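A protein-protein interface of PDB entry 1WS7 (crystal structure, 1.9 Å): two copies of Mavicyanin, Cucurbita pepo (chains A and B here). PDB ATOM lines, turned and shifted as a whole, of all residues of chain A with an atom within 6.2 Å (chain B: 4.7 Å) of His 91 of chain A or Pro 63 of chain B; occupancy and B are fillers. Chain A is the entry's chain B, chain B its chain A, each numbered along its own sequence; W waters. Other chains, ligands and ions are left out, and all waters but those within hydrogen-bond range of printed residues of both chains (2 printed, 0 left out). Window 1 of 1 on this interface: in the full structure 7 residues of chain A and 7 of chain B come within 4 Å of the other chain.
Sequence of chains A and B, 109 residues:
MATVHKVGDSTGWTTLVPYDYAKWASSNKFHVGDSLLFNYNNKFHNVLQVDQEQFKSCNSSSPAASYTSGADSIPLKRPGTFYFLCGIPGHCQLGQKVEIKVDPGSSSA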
ATOM      1  N   THR A  15      20.526 -10.587  28.469  1.00  0.00           N
ATOM      2  CA  THR A  15      19.494 -11.032  29.408  1.00  0.00           C
ATOM      3  C   THR A  15      20.066 -12.164  30.266  1.00  0.00           C
ATOM      4  O   THR A  15      19.374 -12.699  31.133  1.00  0.00           O
ATOM      5  CB  THR A  15      18.209 -11.569  28.709  1.00  0.00           C
ATOM      6  OG1 THR A  15      18.542 -12.674  27.859  1.00  0.00           O
ATOM      7  CG2 THR A  15      17.533 -10.469  27.898  1.00  0.00           C
ATOM      8  N   PHE A  44      21.453 -13.527  18.977  1.00  0.00           N
ATOM      9  CA  PHE A  44      20.360 -13.662  19.944  1.00  0.00           C
ATOM     10  C   PHE A  44      19.664 -12.404  20.458  1.00  0.00           C
ATOM     11  O   PHE A  44      18.725 -12.507  21.252  1.00  0.00           O
ATOM     12  CB  PHE A  44      20.870 -14.454  21.154  1.00  0.00           C
ATOM     13  CG  PHE A  44      21.563 -15.741  20.794  1.00  0.00           C
ATOM     14  CD1 PHE A  44      22.858 -15.994  21.237  1.00  0.00           C
ATOM     15  CD2 PHE A  44      20.922 -16.701  20.021  1.00  0.00           C
ATOM     16  CE1 PHE A  44      23.506 -17.187  20.915  1.00  0.00           C
ATOM     17  CE2 PHE A  44      21.559 -17.898  19.693  1.00  0.00           C
ATOM     18  CZ  PHE A  44      22.851 -18.141  20.138  1.00  0.00           C
ATOM     19  N   HIS A  45      20.126 -11.233  20.029  1.00  0.00           N
ATOM     20  CA  HIS A  45      19.539  -9.967  20.464  1.00  0.00           C
ATOM     21  C   HIS A  45      19.536  -8.972  19.316  1.00  0.00           C
ATOM     22  O   HIS A  45      20.130  -9.216  18.268  1.00  0.00           O
ATOM     23  CB  HIS A  45      20.373  -9.345  21.590  1.00  0.00           C
ATOM     24  CG  HIS A  45      20.537 -10.221  22.788  1.00  0.00           C
ATOM     25  ND1 HIS A  45      19.522 -10.444  23.692  1.00  0.00           N
ATOM     26  CD2 HIS A  45      21.600 -10.934  23.232  1.00  0.00           C
ATOM     27  CE1 HIS A  45      19.952 -11.254  24.643  1.00  0.00           C
ATOM     28  NE2 HIS A  45      21.210 -11.566  24.386  1.00  0.00           N
ATOM     29  N   CYS A  58       6.693  -2.633  25.988  1.00  0.00           N
ATOM     30  CA  CYS A  58       7.652  -3.573  25.419  1.00  0.00           C
ATOM     31  C   CYS A  58       7.172  -4.055  24.054  1.00  0.00           C
ATOM     32  O   CYS A  58       7.315  -5.230  23.705  1.00  0.00           O
ATOM     33  CB  CYS A  58       7.850  -4.769  26.348  1.00  0.00           C
ATOM     34  SG  CYS A  58       9.176  -4.570  27.579  1.00  0.00           S
ATOM     35  N   CYS A  86      15.228  -4.581  23.161  1.00  0.00           N
ATOM     36  CA  CYS A  86      15.529  -5.734  22.326  1.00  0.00           C
ATOM     37  C   CYS A  86      14.180  -6.327  21.959  1.00  0.00           C
ATOM     38  O   CYS A  86      13.338  -6.546  22.835  1.00  0.00           O
ATOM     39  CB  CYS A  86      16.356  -6.773  23.085  1.00  0.00           C
ATOM     40  SG  CYS A  86      16.610  -8.290  22.124  1.00  0.00           S
ATOM     41  N   GLY A  87      13.974  -6.580  20.672  1.00  0.00           N
ATOM     42  CA  GLY A  87      12.704  -7.129  20.225  1.00  0.00           C
ATOM     43  C   GLY A  87      12.548  -8.635  20.330  1.00  0.00           C
ATOM     44  O   GLY A  87      11.465  -9.164  20.079  1.00  0.00           O
ATOM     45  N   ILE A  88      13.615  -9.335  20.695  1.00  0.00           N
ATOM     46  CA  ILE A  88      13.543 -10.786  20.823  1.00  0.00           C
ATOM     47  C   ILE A  88      12.461 -11.132  21.846  1.00  0.00           C
ATOM     48  O   ILE A  88      12.415 -10.556  22.932  1.00  0.00           O
ATOM     49  CB  ILE A  88      14.905 -11.357  21.255  1.00  0.00           C
ATOM     50  CG1 ILE A  88      15.960 -10.994  20.202  1.00  0.00           C
ATOM     51  CG2 ILE A  88      14.821 -12.867  21.424  1.00  0.00           C
ATOM     52  CD1 ILE A  88      15.625 -11.475  18.795  1.00  0.00           C
ATOM     53  N   PRO A  89      11.573 -12.082  21.507  1.00  0.00           N
ATOM     54  CA  PRO A  89      10.478 -12.501  22.387  1.00  0.00           C
ATOM     55  C   PRO A  89      10.792 -12.561  23.877  1.00  0.00           C
ATOM     56  O   PRO A  89      11.627 -13.353  24.319  1.00  0.00           O
ATOM     57  CB  PRO A  89      10.085 -13.860  21.815  1.00  0.00           C
ATOM     58  CG  PRO A  89      10.296 -13.650  20.345  1.00  0.00           C
ATOM     59  CD  PRO A  89      11.639 -12.949  20.315  1.00  0.00           C
ATOM     60  N   GLY A  90      10.119 -11.699  24.638  1.00  0.00           N
ATOM     61  CA  GLY A  90      10.288 -11.670  26.083  1.00  0.00           C
ATOM     62  C   GLY A  90      11.514 -10.991  26.670  1.00  0.00           C
ATOM     63  O   GLY A  90      11.573 -10.776  27.880  1.00  0.00           O
ATOM     64  N   HIS A  91      12.495 -10.646  25.843  1.00  0.00           N
ATOM     65  CA  HIS A  91      13.698 -10.009  26.378  1.00  0.00           C
ATOM     66  C   HIS A  91      13.450  -8.637  26.993  1.00  0.00           C
ATOM     67  O   HIS A  91      13.993  -8.310  28.050  1.00  0.00           O
ATOM     68  CB  HIS A  91      14.779  -9.914  25.298  1.00  0.00           C
ATOM     69  CG  HIS A  91      15.437 -11.225  24.998  1.00  0.00           C
ATOM     70  ND1 HIS A  91      16.589 -11.326  24.249  1.00  0.00           N
ATOM     71  CD2 HIS A  91      15.096 -12.490  25.338  1.00  0.00           C
ATOM     72  CE1 HIS A  91      16.930 -12.598  24.137  1.00  0.00           C
ATOM     73  NE2 HIS A  91      16.040 -13.326  24.789  1.00  0.00           N
ATOM     74  N   CYS A  92      12.633  -7.828  26.335  1.00  0.00           N
ATOM     75  CA  CYS A  92      12.325  -6.501  26.854  1.00  0.00           C
ATOM     76  C   CYS A  92      11.654  -6.642  28.219  1.00  0.00           C
ATOM     77  O   CYS A  92      11.923  -5.873  29.142  1.00  0.00           O
ATOM     78  CB  CYS A  92      11.389  -5.780  25.893  1.00  0.00           C
ATOM     79  SG  CYS A  92      10.808  -4.143  26.438  1.00  0.00           S
ATOM     80  N   GLN A  93      10.784  -7.639  28.338  1.00  0.00           N
ATOM     81  CA  GLN A  93      10.076  -7.874  29.584  1.00  0.00           C
ATOM     82  C   GLN A  93      11.038  -8.326  30.685  1.00  0.00           C
ATOM     83  O   GLN A  93      10.773  -8.122  31.873  1.00  0.00           O
ATOM     84  CB  GLN A  93       8.954  -8.896  29.368  1.00  0.00           C
ATOM     85  CG  GLN A  93       7.852  -8.409  28.418  1.00  0.00           C
ATOM     86  CD  GLN A  93       8.156  -8.656  26.937  1.00  0.00           C
ATOM     87  OE1 GLN A  93       9.248  -8.357  26.445  1.00  0.00           O
ATOM     88  NE2 GLN A  93       7.174  -9.195  26.219  1.00  0.00           N
ATOM     89  N   LEU A  94      12.162  -8.921  30.290  1.00  0.00           N
ATOM     90  CA  LEU A  94      13.162  -9.368  31.256  1.00  0.00           C
ATOM     91  C   LEU A  94      14.048  -8.204  31.696  1.00  0.00           C
ATOM     92  O   LEU A  94      14.959  -8.381  32.509  1.00  0.00           O
ATOM     93  CB  LEU A  94      14.036 -10.476  30.661  1.00  0.00           C
ATOM     94  CG  LEU A  94      13.376 -11.842  30.455  1.00  0.00           C
ATOM     95  CD1 LEU A  94      14.373 -12.796  29.813  1.00  0.00           C
ATOM     96  CD2 LEU A  94      12.903 -12.395  31.795  1.00  0.00           C
ATOM     97  N   GLY A  95      13.791  -7.023  31.139  1.00  0.00           N
ATOM     98  CA  GLY A  95      14.562  -5.849  31.511  1.00  0.00           C
ATOM     99  C   GLY A  95      15.503  -5.284  30.465  1.00  0.00           C
ATOM    100  O   GLY A  95      16.160  -4.268  30.709  1.00  0.00           O
ATOM    101  N   GLN A  96      15.577  -5.920  29.299  1.00  0.00           N
ATOM    102  CA  GLN A  96      16.477  -5.438  28.254  1.00  0.00           C
ATOM    103  C   GLN A  96      15.873  -4.263  27.482  1.00  0.00           C
ATOM    104  O   GLN A  96      15.385  -4.411  26.357  1.00  0.00           O
ATOM    105  CB  GLN A  96      16.838  -6.579  27.304  1.00  0.00           C
ATOM    106  CG  GLN A  96      18.055  -6.289  26.430  1.00  0.00           C
ATOM    107  CD  GLN A  96      18.472  -7.495  25.615  1.00  0.00           C
ATOM    108  OE1 GLN A  96      17.730  -8.469  25.518  1.00  0.00           O
ATOM    109  NE2 GLN A  96      19.664  -7.433  25.016  1.00  0.00           N
ATOM    110  N   LYS A  97      15.916  -3.094  28.112  1.00  0.00           N
ATOM    111  CA  LYS A  97      15.386  -1.861  27.540  1.00  0.00           C
ATOM    112  C   LYS A  97      16.071  -0.706  28.259  1.00  0.00           C
ATOM    113  O   LYS A  97      16.475  -0.839  29.417  1.00  0.00           O
ATOM    114  CB  LYS A  97      13.876  -1.767  27.778  1.00  0.00           C
ATOM    115  CG  LYS A  97      13.507  -1.913  29.247  1.00  0.00           C
ATOM    116  CD  LYS A  97      12.153  -1.309  29.586  1.00  0.00           C
ATOM    117  CE  LYS A  97      11.009  -1.959  28.841  1.00  0.00           C
ATOM    118  NZ  LYS A  97       9.705  -1.429  29.341  1.00  0.00           N
ATOM    119  N   LEU B  48      17.856 -24.785  24.363  1.00  0.00           N
ATOM    120  CA  LEU B  48      17.649 -23.392  24.735  1.00  0.00           C
ATOM    121  C   LEU B  48      18.344 -23.062  26.045  1.00  0.00           C
ATOM    122  O   LEU B  48      18.255 -23.819  27.011  1.00  0.00           O
ATOM    123  CB  LEU B  48      16.152 -23.099  24.888  1.00  0.00           C
ATOM    124  CG  LEU B  48      15.199 -23.500  23.761  1.00  0.00           C
ATOM    125  CD1 LEU B  48      13.777 -23.082  24.139  1.00  0.00           C
ATOM    126  CD2 LEU B  48      15.624 -22.841  22.454  1.00  0.00           C
ATOM    127  N   GLN B  49      19.046 -21.934  26.070  1.00  0.00           N
ATOM    128  CA  GLN B  49      19.718 -21.500  27.283  1.00  0.00           C
ATOM    129  C   GLN B  49      18.738 -20.558  27.978  1.00  0.00           C
ATOM    130  O   GLN B  49      18.211 -19.631  27.357  1.00  0.00           O
ATOM    131  CB  GLN B  49      21.023 -20.762  26.961  1.00  0.00           C
ATOM    132  CG  GLN B  49      21.707 -20.189  28.203  1.00  0.00           C
ATOM    133  CD  GLN B  49      23.047 -19.544  27.911  1.00  0.00           C
ATOM    134  OE1 GLN B  49      23.333 -19.148  26.779  1.00  0.00           O
ATOM    135  NE2 GLN B  49      23.872 -19.414  28.941  1.00  0.00           N
ATOM    136  N   VAL B  50      18.484 -20.814  29.257  1.00  0.00           N
ATOM    137  CA  VAL B  50      17.549 -20.013  30.041  1.00  0.00           C
ATOM    138  C   VAL B  50      18.150 -19.662  31.405  1.00  0.00           C
ATOM    139  O   VAL B  50      19.277 -20.051  31.712  1.00  0.00           O
ATOM    140  CB  VAL B  50      16.231 -20.795  30.278  1.00  0.00           C
ATOM    141  CG1 VAL B  50      15.617 -21.210  28.945  1.00  0.00           C
ATOM    142  CG2 VAL B  50      16.506 -22.027  31.137  1.00  0.00           C
ATOM    143  N   SER B  60      10.047 -21.895  28.329  1.00  0.00           N
ATOM    144  CA  SER B  60      10.877 -21.760  27.136  1.00  0.00           C
ATOM    145  C   SER B  60      10.420 -20.624  26.221  1.00  0.00           C
ATOM    146  O   SER B  60      10.809 -20.563  25.054  1.00  0.00           O
ATOM    147  CB  SER B  60      10.855 -23.075  26.357  1.00  0.00           C
ATOM    148  OG  SER B  60       9.522 -23.448  26.054  1.00  0.00           O
ATOM    149  N   SER B  61       9.606 -19.717  26.753  1.00  0.00           N
ATOM    150  CA  SER B  61       9.079 -18.613  25.954  1.00  0.00           C
ATOM    151  C   SER B  61      10.048 -17.471  25.670  1.00  0.00           C
ATOM    152  O   SER B  61       9.827 -16.684  24.744  1.00  0.00           O
ATOM    153  CB  SER B  61       7.832 -18.038  26.626  1.00  0.00           C
ATOM    154  OG  SER B  61       8.177 -17.362  27.823  1.00  0.00           O
ATOM    155  N   SER B  62      11.116 -17.365  26.453  1.00  0.00           N
ATOM    156  CA  SER B  62      12.068 -16.275  26.244  1.00  0.00           C
ATOM    157  C   SER B  62      13.503 -16.684  26.555  1.00  0.00           C
ATOM    158  O   SER B  62      14.120 -16.159  27.485  1.00  0.00           O
ATOM    159  CB  SER B  62      11.675 -15.076  27.114  1.00  0.00           C
ATOM    160  OG  SER B  62      12.471 -13.941  26.803  1.00  0.00           O
ATOM    161  N   PRO B  63      14.059 -17.620  25.770  1.00  0.00           N
ATOM    162  CA  PRO B  63      15.432 -18.093  25.976  1.00  0.00           C
ATOM    163  C   PRO B  63      16.500 -17.045  25.681  1.00  0.00           C
ATOM    164  O   PRO B  63      16.307 -16.167  24.838  1.00  0.00           O
ATOM    165  CB  PRO B  63      15.522 -19.297  25.039  1.00  0.00           C
ATOM    166  CG  PRO B  63      14.608 -18.906  23.908  1.00  0.00           C
ATOM    167  CD  PRO B  63      13.415 -18.343  24.659  1.00  0.00           C
ATOM    168  N   ALA B  64      17.627 -17.156  26.378  1.00  0.00           N
ATOM    169  CA  ALA B  64      18.740 -16.232  26.206  1.00  0.00           C
ATOM    170  C   ALA B  64      19.564 -16.603  24.974  1.00  0.00           C
ATOM    171  O   ALA B  64      20.224 -15.755  24.376  1.00  0.00           O
ATOM    172  CB  ALA B  64      19.618 -16.242  27.453  1.00  0.00           C
ATOM    173  N   ALA B  65      19.522 -17.880  24.607  1.00  0.00           N
ATOM    174  CA  ALA B  65      20.250 -18.377  23.444  1.00  0.00           C
ATOM    175  C   ALA B  65      19.539 -19.630  22.949  1.00  0.00           C
ATOM    176  O   ALA B  65      18.845 -20.296  23.715  1.00  0.00           O
ATOM    177  CB  ALA B  65      21.690 -18.698  23.818  1.00  0.00           C
HETATM  178  O   HOH W   1       8.127 -14.479  25.293  1.00  0.00           O
HETATM  179  O   HOH W   2      16.534 -14.544  27.992  1.00  0.00           O
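The backbone carbonyl oxygen of Gly 90 of chain A sits close to the side-chain hydroxyl of Ser 62 of chain B (3.5 Å).
The side-chain hydroxyl of Ser 62 of chain B sits close to the backbone NH of His 91 of chain A, at 3.4 Å.
The side-chain hydroxyl of Ser 62 of chain B sits at hydrogen-bond distance from the backbone carbonyl oxygen of Pro 89 of chain A.
The backbone carbonyl oxygen of Pro 63 of chain B is in hydrogen-bond range of a ring nitrogen (NE2) of His 91 of chain A (2.9 Å).
Water W2 lies within hydrogen-bond range of the side-chain hydroxyl (OG1) of Thr 15 of chain A (2.7 Å), the backbone carbonyl oxygen (O) of Ser 62 of chain B (2.9 Å), the backbone NH (N) of Ala 64 of chain B (3.3 Å) and a ring nitrogen (NE2) of His 91 of chain A (3.5 Å).
Water W1 bridges the backbone carbonyl oxygen of Ser 61 of chain B (2.8 Å) and the backbone NH of Gly 90 of chain A (3.5 Å).
Of the printed residues of chain B, Phe 44 of chain A touches Ala 64 and Ala 65.
Of the printed residues of chain B, Pro 89 of chain A touches Ser 61 and Ser 62.
Of chain B, only Ser 62 and Pro 63 come within 4 Å of His 91 of chain A.
Of the printed residues of chain B, Leu 94 of chain A touches Ser 62.
Gly 95 of chain A touches none of the printed residues of chain B.
Printed residues of chain A within 4 Å of Ser 62 of chain B: Pro 89, Gly 90, His 91 and Leu 94.
The nearest residue of chain B that does not touch His 91 of chain A is Ala 64 of chain B (4.2 Å).
The nearest residue of chain A that does not touch Pro 63 of chain B is Ile 88 of chain A (5.0 Å).
OG1 of Thr 15 of chain A touches CB of Ala 64 of chain B, at 3.7 Å.
CB of Phe 44 of chain A touches O of Ala 64 of chain B, 3.5 Å away.
Phe 44 of chain A touches Ala 65 of chain B.
Ser 61 of chain B touches Pro 89 of chain A (O to O, 3.8 Å).
Ser 62 of chain B touches Leu 94 of chain A (OG to CD1, 3.7 Å).
Hydrophobic or aromatic side chains of chain A that line the printed part of chain B: Phe 44, His 91 and Leu 94.
Among the printed residues, 9 pairs touch across the chains.
Among the printed residues, no Asp or Glu carboxylate lies within 4 Å of a Lys or Arg side-chain nitrogen of the other chain.
The backbone carbonyl oxygen (O) of Ala 65 of chain B lies within hydrogen-bond range of the backbone NH (N) of Gln 49 of chain B (2.9 Å).
SG of Cys 58 of chain A forms a disulfide with SG of Cys 92 of chain A (2.0 Å).
The backbone carbonyl oxygen (O) of Gln 49 of chain B sits at hydrogen-bond distance from the backbone NH (N) of Ala 64 of chain B (2.7 Å).
No position is printed for both chains.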
